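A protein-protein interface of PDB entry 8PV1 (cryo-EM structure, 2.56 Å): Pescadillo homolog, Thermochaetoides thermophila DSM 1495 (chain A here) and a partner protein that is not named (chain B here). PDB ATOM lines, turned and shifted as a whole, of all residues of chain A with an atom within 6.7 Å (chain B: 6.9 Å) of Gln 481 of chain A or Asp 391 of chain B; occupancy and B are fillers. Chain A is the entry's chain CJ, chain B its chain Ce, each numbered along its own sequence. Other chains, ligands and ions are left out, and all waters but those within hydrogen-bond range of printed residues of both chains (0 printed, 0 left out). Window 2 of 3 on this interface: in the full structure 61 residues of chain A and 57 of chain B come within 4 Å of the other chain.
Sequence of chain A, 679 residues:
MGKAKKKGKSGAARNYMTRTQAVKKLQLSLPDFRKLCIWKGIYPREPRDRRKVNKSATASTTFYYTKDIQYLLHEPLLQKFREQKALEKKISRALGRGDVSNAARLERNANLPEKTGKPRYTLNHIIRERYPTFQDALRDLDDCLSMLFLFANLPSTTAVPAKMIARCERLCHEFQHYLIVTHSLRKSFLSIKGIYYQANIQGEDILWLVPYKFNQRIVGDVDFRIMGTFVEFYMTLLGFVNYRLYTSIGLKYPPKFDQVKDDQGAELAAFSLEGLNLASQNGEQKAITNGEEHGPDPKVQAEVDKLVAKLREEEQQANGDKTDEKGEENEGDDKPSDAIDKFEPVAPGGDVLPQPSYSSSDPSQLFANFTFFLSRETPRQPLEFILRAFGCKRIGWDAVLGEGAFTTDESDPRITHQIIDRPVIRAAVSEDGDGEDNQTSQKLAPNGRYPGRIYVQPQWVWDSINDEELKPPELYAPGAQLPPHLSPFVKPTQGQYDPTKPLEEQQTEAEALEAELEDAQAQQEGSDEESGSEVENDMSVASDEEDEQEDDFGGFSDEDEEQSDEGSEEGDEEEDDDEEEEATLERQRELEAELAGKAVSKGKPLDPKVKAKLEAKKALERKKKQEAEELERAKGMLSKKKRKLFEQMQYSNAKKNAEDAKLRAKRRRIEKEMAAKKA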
ATOM      1  N   ASP A 421     -15.688  22.436  28.720  1.00  0.00           N
ATOM      2  CA  ASP A 421     -14.788  22.687  27.601  1.00  0.00           C
ATOM      3  C   ASP A 421     -13.419  23.163  28.072  1.00  0.00           C
ATOM      4  O   ASP A 421     -12.842  24.081  27.480  1.00  0.00           O
ATOM      5  CB  ASP A 421     -15.404  23.711  26.645  1.00  0.00           C
ATOM      6  CG  ASP A 421     -14.937  23.530  25.215  1.00  0.00           C
ATOM      7  OD1 ASP A 421     -14.095  22.642  24.970  1.00  0.00           O
ATOM      8  OD2 ASP A 421     -15.410  24.280  24.337  1.00  0.00           O
ATOM      9  N   GLN A 457     -18.705  17.434  25.641  1.00  0.00           N
ATOM     10  CA  GLN A 457     -18.390  18.696  24.992  1.00  0.00           C
ATOM     11  C   GLN A 457     -19.630  19.255  24.304  1.00  0.00           C
ATOM     12  O   GLN A 457     -20.582  18.516  24.038  1.00  0.00           O
ATOM     13  CB  GLN A 457     -17.255  18.489  23.989  1.00  0.00           C
ATOM     14  CG  GLN A 457     -16.021  17.847  24.601  1.00  0.00           C
ATOM     15  CD  GLN A 457     -14.780  18.040  23.757  1.00  0.00           C
ATOM     16  OE1 GLN A 457     -14.633  19.052  23.074  1.00  0.00           O
ATOM     17  NE2 GLN A 457     -13.879  17.067  23.798  1.00  0.00           N
ATOM     18  N   GLU A 474     -18.859   8.641  24.737  1.00  0.00           N
ATOM     19  CA  GLU A 474     -17.420   8.403  24.803  1.00  0.00           C
ATOM     20  C   GLU A 474     -16.678   9.078  23.658  1.00  0.00           C
ATOM     21  O   GLU A 474     -15.477   9.349  23.774  1.00  0.00           O
ATOM     22  CB  GLU A 474     -17.134   6.898  24.822  1.00  0.00           C
ATOM     23  CG  GLU A 474     -17.439   6.157  23.524  1.00  0.00           C
ATOM     24  CD  GLU A 474     -18.893   5.727  23.399  1.00  0.00           C
ATOM     25  OE1 GLU A 474     -19.749   6.238  24.152  1.00  0.00           O
ATOM     26  OE2 GLU A 474     -19.180   4.868  22.538  1.00  0.00           O
ATOM     27  N   LEU A 475     -17.364   9.359  22.548  1.00  0.00           N
ATOM     28  CA  LEU A 475     -16.745  10.102  21.459  1.00  0.00           C
ATOM     29  C   LEU A 475     -16.604  11.582  21.777  1.00  0.00           C
ATOM     30  O   LEU A 475     -15.737  12.249  21.202  1.00  0.00           O
ATOM     31  CB  LEU A 475     -17.547   9.936  20.162  1.00  0.00           C
ATOM     32  CG  LEU A 475     -17.348   8.706  19.264  1.00  0.00           C
ATOM     33  CD1 LEU A 475     -15.929   8.677  18.709  1.00  0.00           C
ATOM     34  CD2 LEU A 475     -17.701   7.384  19.940  1.00  0.00           C
ATOM     35  N   TYR A 476     -17.430  12.103  22.682  1.00  0.00           N
ATOM     36  CA  TYR A 476     -17.415  13.507  23.067  1.00  0.00           C
ATOM     37  C   TYR A 476     -16.812  13.701  24.452  1.00  0.00           C
ATOM     38  O   TYR A 476     -17.205  14.620  25.179  1.00  0.00           O
ATOM     39  CB  TYR A 476     -18.828  14.089  23.004  1.00  0.00           C
ATOM     40  CG  TYR A 476     -19.449  14.017  21.625  1.00  0.00           C
ATOM     41  CD1 TYR A 476     -20.118  12.874  21.200  1.00  0.00           C
ATOM     42  CD2 TYR A 476     -19.363  15.086  20.746  1.00  0.00           C
ATOM     43  CE1 TYR A 476     -20.677  12.799  19.946  1.00  0.00           C
ATOM     44  CE2 TYR A 476     -19.924  15.020  19.485  1.00  0.00           C
ATOM     45  CZ  TYR A 476     -20.580  13.874  19.094  1.00  0.00           C
ATOM     46  OH  TYR A 476     -21.143  13.794  17.842  1.00  0.00           O
ATOM     47  N   ALA A 477     -15.865  12.843  24.826  1.00  0.00           N
ATOM     48  CA  ALA A 477     -15.236  12.887  26.131  1.00  0.00           C
ATOM     49  C   ALA A 477     -14.398  14.156  26.283  1.00  0.00           C
ATOM     50  O   ALA A 477     -13.966  14.746  25.290  1.00  0.00           O
ATOM     51  CB  ALA A 477     -14.363  11.650  26.329  1.00  0.00           C
ATOM     52  N   GLY A 479     -11.342  16.334  26.454  1.00  0.00           N
ATOM     53  CA  GLY A 479     -10.012  16.160  25.916  1.00  0.00           C
ATOM     54  C   GLY A 479      -9.928  15.270  24.696  1.00  0.00           C
ATOM     55  O   GLY A 479      -8.870  15.225  24.056  1.00  0.00           O
ATOM     56  N   ALA A 480     -10.999  14.564  24.352  1.00  0.00           N
ATOM     57  CA  ALA A 480     -10.992  13.683  23.199  1.00  0.00           C
ATOM     58  C   ALA A 480     -11.158  14.479  21.909  1.00  0.00           C
ATOM     59  O   ALA A 480     -11.602  15.631  21.908  1.00  0.00           O
ATOM     60  CB  ALA A 480     -12.100  12.635  23.313  1.00  0.00           C
ATOM     61  N   GLN A 481     -10.788  13.846  20.799  1.00  0.00           N
ATOM     62  CA  GLN A 481     -10.952  14.443  19.478  1.00  0.00           C
ATOM     63  C   GLN A 481     -12.405  14.280  19.052  1.00  0.00           C
ATOM     64  O   GLN A 481     -12.915  13.159  18.973  1.00  0.00           O
ATOM     65  CB  GLN A 481     -10.005  13.791  18.474  1.00  0.00           C
ATOM     66  CG  GLN A 481      -8.548  14.257  18.549  1.00  0.00           C
ATOM     67  CD  GLN A 481      -8.340  15.748  18.294  1.00  0.00           C
ATOM     68  OE1 GLN A 481      -9.159  16.384  17.632  1.00  0.00           O
ATOM     69  NE2 GLN A 481      -7.295  16.324  18.885  1.00  0.00           N
ATOM     70  N   LEU A 482     -13.072  15.397  18.780  1.00  0.00           N
ATOM     71  CA  LEU A 482     -14.481  15.354  18.436  1.00  0.00           C
ATOM     72  C   LEU A 482     -14.679  14.842  17.010  1.00  0.00           C
ATOM     73  O   LEU A 482     -13.821  15.043  16.146  1.00  0.00           O
ATOM     74  CB  LEU A 482     -15.106  16.738  18.580  1.00  0.00           C
ATOM     75  CG  LEU A 482     -15.218  17.274  20.006  1.00  0.00           C
ATOM     76  CD1 LEU A 482     -15.919  18.618  20.015  1.00  0.00           C
ATOM     77  CD2 LEU A 482     -15.954  16.281  20.884  1.00  0.00           C
ATOM     78  N   PRO A 483     -15.793  14.167  16.744  1.00  0.00           N
ATOM     79  CA  PRO A 483     -16.156  13.831  15.363  1.00  0.00           C
ATOM     80  C   PRO A 483     -16.448  15.089  14.567  1.00  0.00           C
ATOM     81  O   PRO A 483     -16.788  16.129  15.150  1.00  0.00           O
ATOM     82  CB  PRO A 483     -17.417  12.966  15.527  1.00  0.00           C
ATOM     83  CG  PRO A 483     -17.372  12.477  16.926  1.00  0.00           C
ATOM     84  CD  PRO A 483     -16.710  13.554  17.720  1.00  0.00           C
ATOM     85  N   TYR B 215     -16.941  24.737  12.136  1.00  0.00           N
ATOM     86  CA  TYR B 215     -15.744  25.054  12.907  1.00  0.00           C
ATOM     87  C   TYR B 215     -14.847  23.831  13.011  1.00  0.00           C
ATOM     88  O   TYR B 215     -13.623  23.960  13.121  1.00  0.00           O
ATOM     89  CB  TYR B 215     -16.117  25.552  14.305  1.00  0.00           C
ATOM     90  CG  TYR B 215     -16.648  24.489  15.240  1.00  0.00           C
ATOM     91  CD1 TYR B 215     -17.986  24.148  15.255  1.00  0.00           C
ATOM     92  CD2 TYR B 215     -15.807  23.885  16.171  1.00  0.00           C
ATOM     93  CE1 TYR B 215     -18.458  23.180  16.118  1.00  0.00           C
ATOM     94  CE2 TYR B 215     -16.271  22.931  17.039  1.00  0.00           C
ATOM     95  CZ  TYR B 215     -17.595  22.584  17.010  1.00  0.00           C
ATOM     96  OH  TYR B 215     -18.055  21.634  17.883  1.00  0.00           O
ATOM     97  N   ASN B 216     -15.449  22.645  12.983  1.00  0.00           N
ATOM     98  CA  ASN B 216     -14.747  21.366  13.030  1.00  0.00           C
ATOM     99  C   ASN B 216     -15.244  20.587  11.821  1.00  0.00           C
ATOM    100  O   ASN B 216     -16.069  19.673  11.945  1.00  0.00           O
ATOM    101  CB  ASN B 216     -15.016  20.640  14.349  1.00  0.00           C
ATOM    102  CG  ASN B 216     -14.332  19.294  14.432  1.00  0.00           C
ATOM    103  OD1 ASN B 216     -13.303  19.065  13.797  1.00  0.00           O
ATOM    104  ND2 ASN B 216     -14.901  18.392  15.221  1.00  0.00           N
ATOM    105  N   LEU B 389      -6.272  25.807  13.044  1.00  0.00           N
ATOM    106  CA  LEU B 389      -7.339  24.930  13.517  1.00  0.00           C
ATOM    107  C   LEU B 389      -7.181  24.617  14.997  1.00  0.00           C
ATOM    108  O   LEU B 389      -6.078  24.347  15.479  1.00  0.00           O
ATOM    109  CB  LEU B 389      -7.379  23.629  12.713  1.00  0.00           C
ATOM    110  CG  LEU B 389      -8.262  23.579  11.463  1.00  0.00           C
ATOM    111  CD1 LEU B 389      -7.718  24.414  10.339  1.00  0.00           C
ATOM    112  CD2 LEU B 389      -8.448  22.138  11.013  1.00  0.00           C
ATOM    113  N   GLU B 390      -8.299  24.655  15.712  1.00  0.00           N
ATOM    114  CA  GLU B 390      -8.356  24.357  17.133  1.00  0.00           C
ATOM    115  C   GLU B 390      -9.255  23.152  17.371  1.00  0.00           C
ATOM    116  O   GLU B 390     -10.085  22.785  16.535  1.00  0.00           O
ATOM    117  CB  GLU B 390      -8.857  25.574  17.919  1.00  0.00           C
ATOM    118  CG  GLU B 390      -7.975  26.802  17.770  1.00  0.00           C
ATOM    119  CD  GLU B 390      -6.682  26.697  18.556  1.00  0.00           C
ATOM    120  OE1 GLU B 390      -6.616  25.878  19.496  1.00  0.00           O
ATOM    121  OE2 GLU B 390      -5.729  27.434  18.230  1.00  0.00           O
ATOM    122  N   ASP B 391      -9.079  22.531  18.535  1.00  0.00           N
ATOM    123  CA  ASP B 391      -9.763  21.288  18.864  1.00  0.00           C
ATOM    124  C   ASP B 391     -10.950  21.491  19.796  1.00  0.00           C
ATOM    125  O   ASP B 391     -11.476  20.508  20.330  1.00  0.00           O
ATOM    126  CB  ASP B 391      -8.777  20.294  19.486  1.00  0.00           C
ATOM    127  CG  ASP B 391      -7.695  19.865  18.516  1.00  0.00           C
ATOM    128  OD1 ASP B 391      -6.714  19.230  18.957  1.00  0.00           O
ATOM    129  OD2 ASP B 391      -7.826  20.160  17.309  1.00  0.00           O
ATOM    130  N   SER B 392     -11.387  22.730  20.009  1.00  0.00           N
ATOM    131  CA  SER B 392     -12.488  23.004  20.919  1.00  0.00           C
ATOM    132  C   SER B 392     -13.306  24.180  20.408  1.00  0.00           C
ATOM    133  O   SER B 392     -12.834  24.986  19.605  1.00  0.00           O
ATOM    134  CB  SER B 392     -11.982  23.297  22.337  1.00  0.00           C
ATOM    135  OG  SER B 392     -11.130  24.427  22.351  1.00  0.00           O
ATOM    136  N   LEU B 393     -14.549  24.259  20.886  1.00  0.00           N
ATOM    137  CA  LEU B 393     -15.403  25.397  20.564  1.00  0.00           C
ATOM    138  C   LEU B 393     -14.961  26.644  21.320  1.00  0.00           C
ATOM    139  O   LEU B 393     -15.198  27.770  20.867  1.00  0.00           O
ATOM    140  CB  LEU B 393     -16.859  25.053  20.881  1.00  0.00           C
ATOM    141  CG  LEU B 393     -17.952  26.075  20.563  1.00  0.00           C
ATOM    142  CD1 LEU B 393     -17.909  26.463  19.097  1.00  0.00           C
ATOM    143  CD2 LEU B 393     -19.318  25.529  20.934  1.00  0.00           C
ATOM    144  N   ARG B 394     -14.319  26.459  22.477  1.00  0.00           N
ATOM    145  CA  ARG B 394     -13.849  27.591  23.271  1.00  0.00           C
ATOM    146  C   ARG B 394     -12.753  28.365  22.548  1.00  0.00           C
ATOM    147  O   ARG B 394     -12.728  29.600  22.583  1.00  0.00           O
ATOM    148  CB  ARG B 394     -13.355  27.094  24.628  1.00  0.00           C
ATOM    149  CG  ARG B 394     -12.725  28.159  25.503  1.00  0.00           C
ATOM    150  CD  ARG B 394     -12.210  27.558  26.794  1.00  0.00           C
ATOM    151  NE  ARG B 394     -11.321  26.430  26.546  1.00  0.00           N
ATOM    152  CZ  ARG B 394     -10.033  26.541  26.255  1.00  0.00           C
ATOM    153  NH1 ARG B 394      -9.440  27.721  26.182  1.00  0.00           N
ATOM    154  NH2 ARG B 394      -9.321  25.440  26.032  1.00  0.00           N
ATOM    155  N   ARG B 395     -11.849  27.660  21.873  1.00  0.00           N
ATOM    156  CA  ARG B 395     -10.743  28.293  21.169  1.00  0.00           C
ATOM    157  C   ARG B 395     -11.079  28.651  19.729  1.00  0.00           C
ATOM    158  O   ARG B 395     -10.165  28.951  18.955  1.00  0.00           O
ATOM    159  CB  ARG B 395      -9.512  27.384  21.192  1.00  0.00           C
ATOM    160  CG  ARG B 395      -8.999  27.066  22.581  1.00  0.00           C
ATOM    161  CD  ARG B 395      -7.483  27.053  22.616  1.00  0.00           C
ATOM    162  NE  ARG B 395      -6.923  28.371  22.339  1.00  0.00           N
ATOM    163  CZ  ARG B 395      -5.761  28.579  21.738  1.00  0.00           C
ATOM    164  NH1 ARG B 395      -5.002  27.574  21.333  1.00  0.00           N
ATOM    165  NH2 ARG B 395      -5.349  29.827  21.536  1.00  0.00           N
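N of Arg 395 of chain B is in hydrogen-bond range of OG of Ser 392 of chain B (3.3 Å).
Of the 11 printed residues of chain A, 4 touch a printed residue of chain B. Printed residues of chain A that touch a printed residue of chain B: Asp 421, Gln 481, Leu 482 and Pro 483. Of the 9 printed residues of chain B, 5 touch a printed residue of chain A. Hydrophobic or aromatic side chains of chain B within 4 Å of the printed part of chain A: Leu 393. Along chain B the printed residues that touch a printed residue of chain A span positions 216 to 394. Among the printed residues, 6 pairs touch across the chains. Among the printed residues, no Asp or Glu carboxylate lies within 4 Å of a Lys or Arg side-chain nitrogen of the other chain.
Gln 481 of chain A touches just one residue of chain B: Asp 391. Asp 391 of chain B touches just one residue of chain A: Gln 481. Of the printed residues of chain A, Ser 392 of chain B touches Asp 421. Of the printed residues of chain A, Leu 393 of chain B touches Asp 421. Of the printed residues of chain B, Asp 421 of chain A touches Ser 392, Leu 393 and Arg 394. Arg 395 of chain B touches none of the printed residues of chain A. The nearest residue of chain B that does not touch Gln 481 of chain A is Asn 216 of chain B (6.1 Å). The nearest printed residue of chain A that does not touch Ser 392 of chain B is Gln 457 of chain A (5.0 Å).
Ser 392 of chain B touches Asp 421 of chain A. Asp 421 of chain A touches Leu 393 of chain B. Asn 216 of chain B touches Leu 482 of chain A.
O of Pro 483 of chain A lies within hydrogen-bond range of ND2 of Asn 216 of chain B (2.9 Å). The side-chain carboxylate of Asp 391 of chain B sits at hydrogen-bond distance from the side-chain amide nitrogen of Gln 481 of chain A (3.0 Å). NE of Arg 394 of chain B lies within hydrogen-bond range of O of Asp 421 of chain A (3.0 Å).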
